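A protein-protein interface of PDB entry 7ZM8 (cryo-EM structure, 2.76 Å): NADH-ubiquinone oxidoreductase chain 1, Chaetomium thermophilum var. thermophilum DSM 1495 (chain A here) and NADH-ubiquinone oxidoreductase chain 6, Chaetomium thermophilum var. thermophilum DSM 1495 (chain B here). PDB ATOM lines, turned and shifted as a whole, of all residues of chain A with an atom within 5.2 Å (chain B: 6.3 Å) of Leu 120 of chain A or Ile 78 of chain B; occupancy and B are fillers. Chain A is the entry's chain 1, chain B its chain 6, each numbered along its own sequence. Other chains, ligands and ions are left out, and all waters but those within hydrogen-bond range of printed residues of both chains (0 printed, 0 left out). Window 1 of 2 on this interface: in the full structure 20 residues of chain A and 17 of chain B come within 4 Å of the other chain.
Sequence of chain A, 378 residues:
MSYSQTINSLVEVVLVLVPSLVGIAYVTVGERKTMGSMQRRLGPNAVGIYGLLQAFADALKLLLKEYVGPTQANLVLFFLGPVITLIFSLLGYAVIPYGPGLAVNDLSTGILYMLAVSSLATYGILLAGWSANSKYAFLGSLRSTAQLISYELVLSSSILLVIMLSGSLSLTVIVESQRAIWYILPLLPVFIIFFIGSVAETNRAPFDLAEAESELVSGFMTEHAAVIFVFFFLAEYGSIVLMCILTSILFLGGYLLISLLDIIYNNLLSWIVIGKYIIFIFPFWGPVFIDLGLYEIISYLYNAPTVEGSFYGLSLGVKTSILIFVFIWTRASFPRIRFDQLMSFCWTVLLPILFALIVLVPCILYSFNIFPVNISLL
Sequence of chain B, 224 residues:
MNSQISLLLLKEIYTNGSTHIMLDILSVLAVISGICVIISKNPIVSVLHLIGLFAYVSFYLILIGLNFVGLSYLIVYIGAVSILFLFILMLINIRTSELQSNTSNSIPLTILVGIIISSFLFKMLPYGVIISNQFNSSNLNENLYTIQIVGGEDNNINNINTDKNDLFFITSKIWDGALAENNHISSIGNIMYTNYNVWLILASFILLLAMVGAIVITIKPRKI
Of the printed residues of chain B, Ala 116 of chain A touches Ile 75. Of chain B, only Ile 78 (3.8 Å) comes within 4 Å of Leu 120 of chain A. Printed residues of chain B within 4 Å of Thr 122 of chain A: Ile 83 (3.8 Å). Printed residues of chain A within 4 Å of Ile 51 of chain B: Tyr 123 (3.4 Å). Ile 78 of chain B touches just these residues of chain A: Leu 120 and Tyr 123. Printed residues of chain A within 4 Å of Ser 82 of chain B: Tyr 123 (2.4 Å). The nearest residue of chain A that does not touch Ile 78 of chain B is Ser 119 of chain A (5.1 Å). The nearest printed residue of chain A that does not touch Gly 79 of chain B is Tyr 123 of chain A (4.8 Å).
CG1 of Ile 75 of chain B touches CA of Ala 116 of chain A, at 3.7 Å. Ser 119 of chain A touches Gly 79 of chain B. Leu 120 of chain A touches Ile 78 of chain B. CD1 of Ile 83 of chain B touches OG1 of Thr 122 of chain A, at 3.8 Å. Ile 51 of chain B touches Tyr 123 of chain A. Tyr 123 of chain A touches Ile 83 of chain B.
Of the 10 printed residues of chain A, 5 touch a printed residue of chain B. Hydrophobic or aromatic side chains of chain B within 4 Å of the printed part of chain A: Ile 51, Ile 75, Ile 78 and Ile 83.
O of Ala 116 of chain A is in hydrogen-bond range of OG of Ser 119 of chain A (2.6 Å). O of Ser 119 of chain A lies within hydrogen-bond range of OG1 of Thr 122 of chain A (2.8 Å). The backbone carbonyl oxygen (O) of Leu 74 of chain B is in hydrogen-bond range of the backbone NH (N) of Gly 79 of chain B (3.1 Å). The backbone carbonyl oxygen (O) of Tyr 77 of chain B is in hydrogen-bond range of the backbone NH (N) of Ser 82 of chain B, 2.9 Å away. OG of Ser 82 of chain B is in hydrogen-bond range of O of Ile 78 of chain B (2.8 Å).
The side-chain hydroxyl (OH) of Tyr 123 of chain A lies within hydrogen-bond range of the backbone carbonyl oxygen (O) of Ile 78 of chain B, at 2.7 Å. The side-chain hydroxyl (OH) of Tyr 123 of chain A lies close to the side-chain hydroxyl (OG) of Ser 82 of chain B (2.4 Å).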
ATOM      1  N   PHE A  88      26.472  11.525  25.217  1.00  0.00           N
ATOM      2  CA  PHE A  88      25.447  10.482  25.479  1.00  0.00           C
ATOM      3  C   PHE A  88      24.441  10.979  26.517  1.00  0.00           C
ATOM      4  O   PHE A  88      23.248  10.646  26.402  1.00  0.00           O
ATOM      5  CB  PHE A  88      26.092   9.182  25.962  1.00  0.00           C
ATOM      6  CG  PHE A  88      26.965   8.473  24.959  1.00  0.00           C
ATOM      7  CD1 PHE A  88      26.813   8.689  23.600  1.00  0.00           C
ATOM      8  CD2 PHE A  88      27.932   7.575  25.381  1.00  0.00           C
ATOM      9  CE1 PHE A  88      27.619   8.035  22.684  1.00  0.00           C
ATOM     10  CE2 PHE A  88      28.736   6.918  24.462  1.00  0.00           C
ATOM     11  CZ  PHE A  88      28.578   7.149  23.116  1.00  0.00           C
ATOM     12  N   ALA A 116      18.615   2.527  23.938  1.00  0.00           N
ATOM     13  CA  ALA A 116      19.937   2.530  23.269  1.00  0.00           C
ATOM     14  C   ALA A 116      20.909   3.498  23.955  1.00  0.00           C
ATOM     15  O   ALA A 116      22.081   3.123  24.142  1.00  0.00           O
ATOM     16  CB  ALA A 116      19.783   2.848  21.804  1.00  0.00           C
ATOM     17  N   VAL A 117      20.419   4.673  24.361  1.00  0.00           N
ATOM     18  CA  VAL A 117      21.295   5.696  25.006  1.00  0.00           C
ATOM     19  C   VAL A 117      21.701   5.228  26.407  1.00  0.00           C
ATOM     20  O   VAL A 117      22.807   5.586  26.840  1.00  0.00           O
ATOM     21  CB  VAL A 117      20.730   7.132  24.964  1.00  0.00           C
ATOM     22  CG1 VAL A 117      20.441   7.594  23.543  1.00  0.00           C
ATOM     23  CG2 VAL A 117      19.522   7.340  25.861  1.00  0.00           C
ATOM     24  N   SER A 118      20.837   4.465  27.082  1.00  0.00           N
ATOM     25  CA  SER A 118      21.147   3.919  28.429  1.00  0.00           C
ATOM     26  C   SER A 118      22.247   2.862  28.334  1.00  0.00           C
ATOM     27  O   SER A 118      23.145   2.856  29.197  1.00  0.00           O
ATOM     28  CB  SER A 118      19.918   3.338  29.050  1.00  0.00           C
ATOM     29  OG  SER A 118      20.112   3.135  30.441  1.00  0.00           O
ATOM     30  N   SER A 119      22.168   1.998  27.322  1.00  0.00           N
ATOM     31  CA  SER A 119      23.173   0.922  27.146  1.00  0.00           C
ATOM     32  C   SER A 119      24.541   1.557  26.879  1.00  0.00           C
ATOM     33  O   SER A 119      25.546   1.019  27.375  1.00  0.00           O
ATOM     34  CB  SER A 119      22.746  -0.025  26.059  1.00  0.00           C
ATOM     35  OG  SER A 119      22.643   0.638  24.810  1.00  0.00           O
ATOM     36  N   LEU A 120      24.575   2.649  26.111  1.00  0.00           N
ATOM     37  CA  LEU A 120      25.843   3.374  25.825  1.00  0.00           C
ATOM     38  C   LEU A 120      26.420   3.957  27.117  1.00  0.00           C
ATOM     39  O   LEU A 120      27.655   4.015  27.227  1.00  0.00           O
ATOM     40  CB  LEU A 120      25.562   4.477  24.802  1.00  0.00           C
ATOM     41  CG  LEU A 120      25.369   4.007  23.363  1.00  0.00           C
ATOM     42  CD1 LEU A 120      24.731   5.098  22.518  1.00  0.00           C
ATOM     43  CD2 LEU A 120      26.694   3.570  22.761  1.00  0.00           C
ATOM     44  N   ALA A 121      25.566   4.381  28.046  1.00  0.00           N
ATOM     45  CA  ALA A 121      26.016   5.048  29.291  1.00  0.00           C
ATOM     46  C   ALA A 121      26.918   4.146  30.137  1.00  0.00           C
ATOM     47  O   ALA A 121      27.776   4.695  30.850  1.00  0.00           O
ATOM     48  CB  ALA A 121      24.812   5.490  30.079  1.00  0.00           C
ATOM     49  N   THR A 122      26.734   2.826  30.073  1.00  0.00           N
ATOM     50  CA  THR A 122      27.511   1.887  30.931  1.00  0.00           C
ATOM     51  C   THR A 122      29.012   2.046  30.673  1.00  0.00           C
ATOM     52  O   THR A 122      29.795   1.792  31.605  1.00  0.00           O
ATOM     53  CB  THR A 122      27.105   0.438  30.648  1.00  0.00           C
ATOM     54  OG1 THR A 122      27.438   0.136  29.293  1.00  0.00           O
ATOM     55  CG2 THR A 122      25.631   0.193  30.881  1.00  0.00           C
ATOM     56  N   TYR A 123      29.396   2.422  29.454  1.00  0.00           N
ATOM     57  CA  TYR A 123      30.827   2.547  29.076  1.00  0.00           C
ATOM     58  C   TYR A 123      31.547   3.595  29.921  1.00  0.00           C
ATOM     59  O   TYR A 123      32.711   3.372  30.256  1.00  0.00           O
ATOM     60  CB  TYR A 123      30.937   2.917  27.600  1.00  0.00           C
ATOM     61  CG  TYR A 123      30.714   1.729  26.710  1.00  0.00           C
ATOM     62  CD1 TYR A 123      31.783   0.966  26.281  1.00  0.00           C
ATOM     63  CD2 TYR A 123      29.437   1.340  26.354  1.00  0.00           C
ATOM     64  CE1 TYR A 123      31.590  -0.145  25.485  1.00  0.00           C
ATOM     65  CE2 TYR A 123      29.225   0.228  25.563  1.00  0.00           C
ATOM     66  CZ  TYR A 123      30.307  -0.509  25.124  1.00  0.00           C
ATOM     67  OH  TYR A 123      30.118  -1.597  24.338  1.00  0.00           O
ATOM     68  N   GLY A 124      30.882   4.707  30.224  1.00  0.00           N
ATOM     69  CA  GLY A 124      31.558   5.783  30.967  1.00  0.00           C
ATOM     70  C   GLY A 124      32.018   5.303  32.324  1.00  0.00           C
ATOM     71  O   GLY A 124      33.148   5.631  32.693  1.00  0.00           O
ATOM     72  N   LEU B  50      35.775  -2.708  17.529  1.00  0.00           N
ATOM     73  CA  LEU B  50      34.572  -3.434  17.155  1.00  0.00           C
ATOM     74  C   LEU B  50      33.325  -2.705  17.634  1.00  0.00           C
ATOM     75  O   LEU B  50      32.307  -2.681  16.936  1.00  0.00           O
ATOM     76  CB  LEU B  50      34.622  -4.850  17.714  1.00  0.00           C
ATOM     77  CG  LEU B  50      33.584  -5.800  17.130  1.00  0.00           C
ATOM     78  CD1 LEU B  50      33.959  -6.172  15.715  1.00  0.00           C
ATOM     79  CD2 LEU B  50      33.452  -7.034  17.988  1.00  0.00           C
ATOM     80  N   ILE B  51      33.381  -2.116  18.829  1.00  0.00           N
ATOM     81  CA  ILE B  51      32.275  -1.287  19.295  1.00  0.00           C
ATOM     82  C   ILE B  51      32.075  -0.109  18.355  1.00  0.00           C
ATOM     83  O   ILE B  51      30.941   0.302  18.083  1.00  0.00           O
ATOM     84  CB  ILE B  51      32.519  -0.826  20.745  1.00  0.00           C
ATOM     85  CG1 ILE B  51      32.703  -2.027  21.663  1.00  0.00           C
ATOM     86  CG2 ILE B  51      31.357   0.000  21.251  1.00  0.00           C
ATOM     87  CD1 ILE B  51      33.355  -1.693  22.971  1.00  0.00           C
ATOM     88  N   GLY B  52      33.168   0.449  17.840  1.00  0.00           N
ATOM     89  CA  GLY B  52      33.047   1.518  16.865  1.00  0.00           C
ATOM     90  C   GLY B  52      32.392   1.060  15.577  1.00  0.00           C
ATOM     91  O   GLY B  52      31.505   1.732  15.052  1.00  0.00           O
ATOM     92  N   PHE B  54      30.286  -1.512  15.061  1.00  0.00           N
ATOM     93  CA  PHE B  54      28.865  -1.889  15.259  1.00  0.00           C
ATOM     94  C   PHE B  54      27.997  -0.638  15.229  1.00  0.00           C
ATOM     95  O   PHE B  54      26.866  -0.739  14.761  1.00  0.00           O
ATOM     96  CB  PHE B  54      28.700  -2.736  16.524  1.00  0.00           C
ATOM     97  CG  PHE B  54      28.875  -4.216  16.309  1.00  0.00           C
ATOM     98  CD1 PHE B  54      27.984  -4.925  15.523  1.00  0.00           C
ATOM     99  CD2 PHE B  54      29.923  -4.903  16.896  1.00  0.00           C
ATOM    100  CE1 PHE B  54      28.140  -6.288  15.329  1.00  0.00           C
ATOM    101  CE2 PHE B  54      30.078  -6.265  16.698  1.00  0.00           C
ATOM    102  CZ  PHE B  54      29.192  -6.955  15.910  1.00  0.00           C
ATOM    103  N   ALA B  55      28.532   0.502  15.667  1.00  0.00           N
ATOM    104  CA  ALA B  55      27.760   1.756  15.713  1.00  0.00           C
ATOM    105  C   ALA B  55      27.708   2.390  14.325  1.00  0.00           C
ATOM    106  O   ALA B  55      26.642   2.864  13.971  1.00  0.00           O
ATOM    107  CB  ALA B  55      28.413   2.680  16.689  1.00  0.00           C
ATOM    108  N   SER B  58      25.021   0.493  12.575  1.00  0.00           N
ATOM    109  CA  SER B  58      23.721   0.789  13.214  1.00  0.00           C
ATOM    110  C   SER B  58      23.205   2.117  12.689  1.00  0.00           C
ATOM    111  O   SER B  58      22.026   2.189  12.346  1.00  0.00           O
ATOM    112  CB  SER B  58      23.897   0.840  14.690  1.00  0.00           C
ATOM    113  OG  SER B  58      24.247  -0.434  15.203  1.00  0.00           O
ATOM    114  N   PHE B  59      24.080   3.110  12.598  1.00  0.00           N
ATOM    115  CA  PHE B  59      23.704   4.453  12.100  1.00  0.00           C
ATOM    116  C   PHE B  59      23.320   4.376  10.627  1.00  0.00           C
ATOM    117  O   PHE B  59      22.355   5.035  10.252  1.00  0.00           O
ATOM    118  CB  PHE B  59      24.841   5.441  12.346  1.00  0.00           C
ATOM    119  CG  PHE B  59      25.239   5.617  13.788  1.00  0.00           C
ATOM    120  CD1 PHE B  59      24.349   5.338  14.812  1.00  0.00           C
ATOM    121  CD2 PHE B  59      26.502   6.073  14.121  1.00  0.00           C
ATOM    122  CE1 PHE B  59      24.719   5.496  16.137  1.00  0.00           C
ATOM    123  CE2 PHE B  59      26.869   6.238  15.447  1.00  0.00           C
ATOM    124  CZ  PHE B  59      25.978   5.948  16.451  1.00  0.00           C
ATOM    125  N   TYR B  73      20.422  -3.463  17.296  1.00  0.00           N
ATOM    126  CA  TYR B  73      21.861  -3.756  17.152  1.00  0.00           C
ATOM    127  C   TYR B  73      22.614  -2.973  18.211  1.00  0.00           C
ATOM    128  O   TYR B  73      23.497  -3.539  18.843  1.00  0.00           O
ATOM    129  CB  TYR B  73      22.370  -3.227  15.815  1.00  0.00           C
ATOM    130  CG  TYR B  73      22.295  -4.157  14.638  1.00  0.00           C
ATOM    131  CD1 TYR B  73      23.134  -5.251  14.522  1.00  0.00           C
ATOM    132  CD2 TYR B  73      21.421  -3.895  13.605  1.00  0.00           C
ATOM    133  CE1 TYR B  73      23.070  -6.089  13.424  1.00  0.00           C
ATOM    134  CE2 TYR B  73      21.332  -4.725  12.507  1.00  0.00           C
ATOM    135  CZ  TYR B  73      22.165  -5.820  12.413  1.00  0.00           C
ATOM    136  OH  TYR B  73      22.061  -6.608  11.311  1.00  0.00           O
ATOM    137  N   LEU B  74      22.264  -1.703  18.388  1.00  0.00           N
ATOM    138  CA  LEU B  74      22.953  -0.847  19.384  1.00  0.00           C
ATOM    139  C   LEU B  74      22.711  -1.388  20.798  1.00  0.00           C
ATOM    140  O   LEU B  74      23.694  -1.521  21.531  1.00  0.00           O
ATOM    141  CB  LEU B  74      22.443   0.591  19.241  1.00  0.00           C
ATOM    142  CG  LEU B  74      23.092   1.440  18.156  1.00  0.00           C
ATOM    143  CD1 LEU B  74      22.446   2.813  18.111  1.00  0.00           C
ATOM    144  CD2 LEU B  74      24.584   1.569  18.396  1.00  0.00           C
ATOM    145  N   ILE B  75      21.473  -1.742  21.138  1.00  0.00           N
ATOM    146  CA  ILE B  75      21.120  -2.304  22.477  1.00  0.00           C
ATOM    147  C   ILE B  75      21.796  -3.661  22.708  1.00  0.00           C
ATOM    148  O   ILE B  75      22.182  -3.926  23.838  1.00  0.00           O
ATOM    149  CB  ILE B  75      19.586  -2.356  22.675  1.00  0.00           C
ATOM    150  CG1 ILE B  75      18.958  -0.964  22.599  1.00  0.00           C
ATOM    151  CG2 ILE B  75      19.203  -3.060  23.965  1.00  0.00           C
ATOM    152  CD1 ILE B  75      17.456  -0.975  22.564  1.00  0.00           C
ATOM    153  N   VAL B  76      21.903  -4.508  21.697  1.00  0.00           N
ATOM    154  CA  VAL B  76      22.445  -5.877  21.922  1.00  0.00           C
ATOM    155  C   VAL B  76      23.962  -5.917  21.747  1.00  0.00           C
ATOM    156  O   VAL B  76      24.633  -6.379  22.663  1.00  0.00           O
ATOM    157  CB  VAL B  76      21.740  -6.904  21.011  1.00  0.00           C
ATOM    158  CG1 VAL B  76      22.414  -8.267  21.038  1.00  0.00           C
ATOM    159  CG2 VAL B  76      20.266  -7.034  21.353  1.00  0.00           C
ATOM    160  N   TYR B  77      24.478  -5.453  20.614  1.00  0.00           N
ATOM    161  CA  TYR B  77      25.939  -5.573  20.369  1.00  0.00           C
ATOM    162  C   TYR B  77      26.758  -4.665  21.274  1.00  0.00           C
ATOM    163  O   TYR B  77      27.685  -5.155  21.912  1.00  0.00           O
ATOM    164  CB  TYR B  77      26.270  -5.457  18.882  1.00  0.00           C
ATOM    165  CG  TYR B  77      25.864  -6.697  18.134  1.00  0.00           C
ATOM    166  CD1 TYR B  77      26.524  -7.894  18.344  1.00  0.00           C
ATOM    167  CD2 TYR B  77      24.787  -6.689  17.270  1.00  0.00           C
ATOM    168  CE1 TYR B  77      26.144  -9.049  17.687  1.00  0.00           C
ATOM    169  CE2 TYR B  77      24.398  -7.834  16.599  1.00  0.00           C
ATOM    170  CZ  TYR B  77      25.077  -9.018  16.811  1.00  0.00           C
ATOM    171  OH  TYR B  77      24.693 -10.147  16.151  1.00  0.00           O
ATOM    172  N   ILE B  78      26.395  -3.393  21.354  1.00  0.00           N
ATOM    173  CA  ILE B  78      27.233  -2.470  22.157  1.00  0.00           C
ATOM    174  C   ILE B  78      26.775  -2.575  23.606  1.00  0.00           C
ATOM    175  O   ILE B  78      27.618  -2.664  24.489  1.00  0.00           O
ATOM    176  CB  ILE B  78      27.172  -1.047  21.576  1.00  0.00           C
ATOM    177  CG1 ILE B  78      27.757  -1.003  20.163  1.00  0.00           C
ATOM    178  CG2 ILE B  78      27.831  -0.031  22.489  1.00  0.00           C
ATOM    179  CD1 ILE B  78      27.808   0.377  19.574  1.00  0.00           C
ATOM    180  N   GLY B  79      25.474  -2.704  23.819  1.00  0.00           N
ATOM    181  CA  GLY B  79      24.956  -2.714  25.185  1.00  0.00           C
ATOM    182  C   GLY B  79      25.307  -3.967  25.940  1.00  0.00           C
ATOM    183  O   GLY B  79      25.509  -3.868  27.171  1.00  0.00           O
ATOM    184  N   ALA B  80      25.366  -5.116  25.269  1.00  0.00           N
ATOM    185  CA  ALA B  80      25.507  -6.348  26.037  1.00  0.00           C
ATOM    186  C   ALA B  80      26.605  -7.272  25.547  1.00  0.00           C
ATOM    187  O   ALA B  80      27.340  -7.824  26.364  1.00  0.00           O
ATOM    188  CB  ALA B  80      24.178  -7.112  26.044  1.00  0.00           C
ATOM    189  N   VAL B  81      26.735  -7.471  24.236  1.00  0.00           N
ATOM    190  CA  VAL B  81      27.711  -8.430  23.733  1.00  0.00           C
ATOM    191  C   VAL B  81      29.125  -7.922  23.973  1.00  0.00           C
ATOM    192  O   VAL B  81      30.004  -8.665  24.421  1.00  0.00           O
ATOM    193  CB  VAL B  81      27.467  -8.724  22.241  1.00  0.00           C
ATOM    194  CG1 VAL B  81      28.548  -9.649  21.701  1.00  0.00           C
ATOM    195  CG2 VAL B  81      26.106  -9.343  22.035  1.00  0.00           C
ATOM    196  N   SER B  82      29.366  -6.648  23.679  1.00  0.00           N
ATOM    197  CA  SER B  82      30.709  -6.108  23.833  1.00  0.00           C
ATOM    198  C   SER B  82      31.062  -5.877  25.297  1.00  0.00           C
ATOM    199  O   SER B  82      32.238  -5.941  25.659  1.00  0.00           O
ATOM    200  CB  SER B  82      30.845  -4.817  23.030  1.00  0.00           C
ATOM    201  OG  SER B  82      29.946  -3.835  23.494  1.00  0.00           O
ATOM    202  N   ILE B  83      30.070  -5.615  26.150  1.00  0.00           N
ATOM    203  CA  ILE B  83      30.336  -5.492  27.581  1.00  0.00           C
ATOM    204  C   ILE B  83      30.842  -6.808  28.148  1.00  0.00           C
ATOM    205  O   ILE B  83      31.796  -6.836  28.932  1.00  0.00           O
ATOM    206  CB  ILE B  83      29.083  -4.991  28.321  1.00  0.00           C
ATOM    207  CG1 ILE B  83      28.775  -3.546  27.927  1.00  0.00           C
ATOM    208  CG2 ILE B  83      29.250  -5.120  29.818  1.00  0.00           C
ATOM    209  CD1 ILE B  83      29.868  -2.572  28.299  1.00  0.00           C
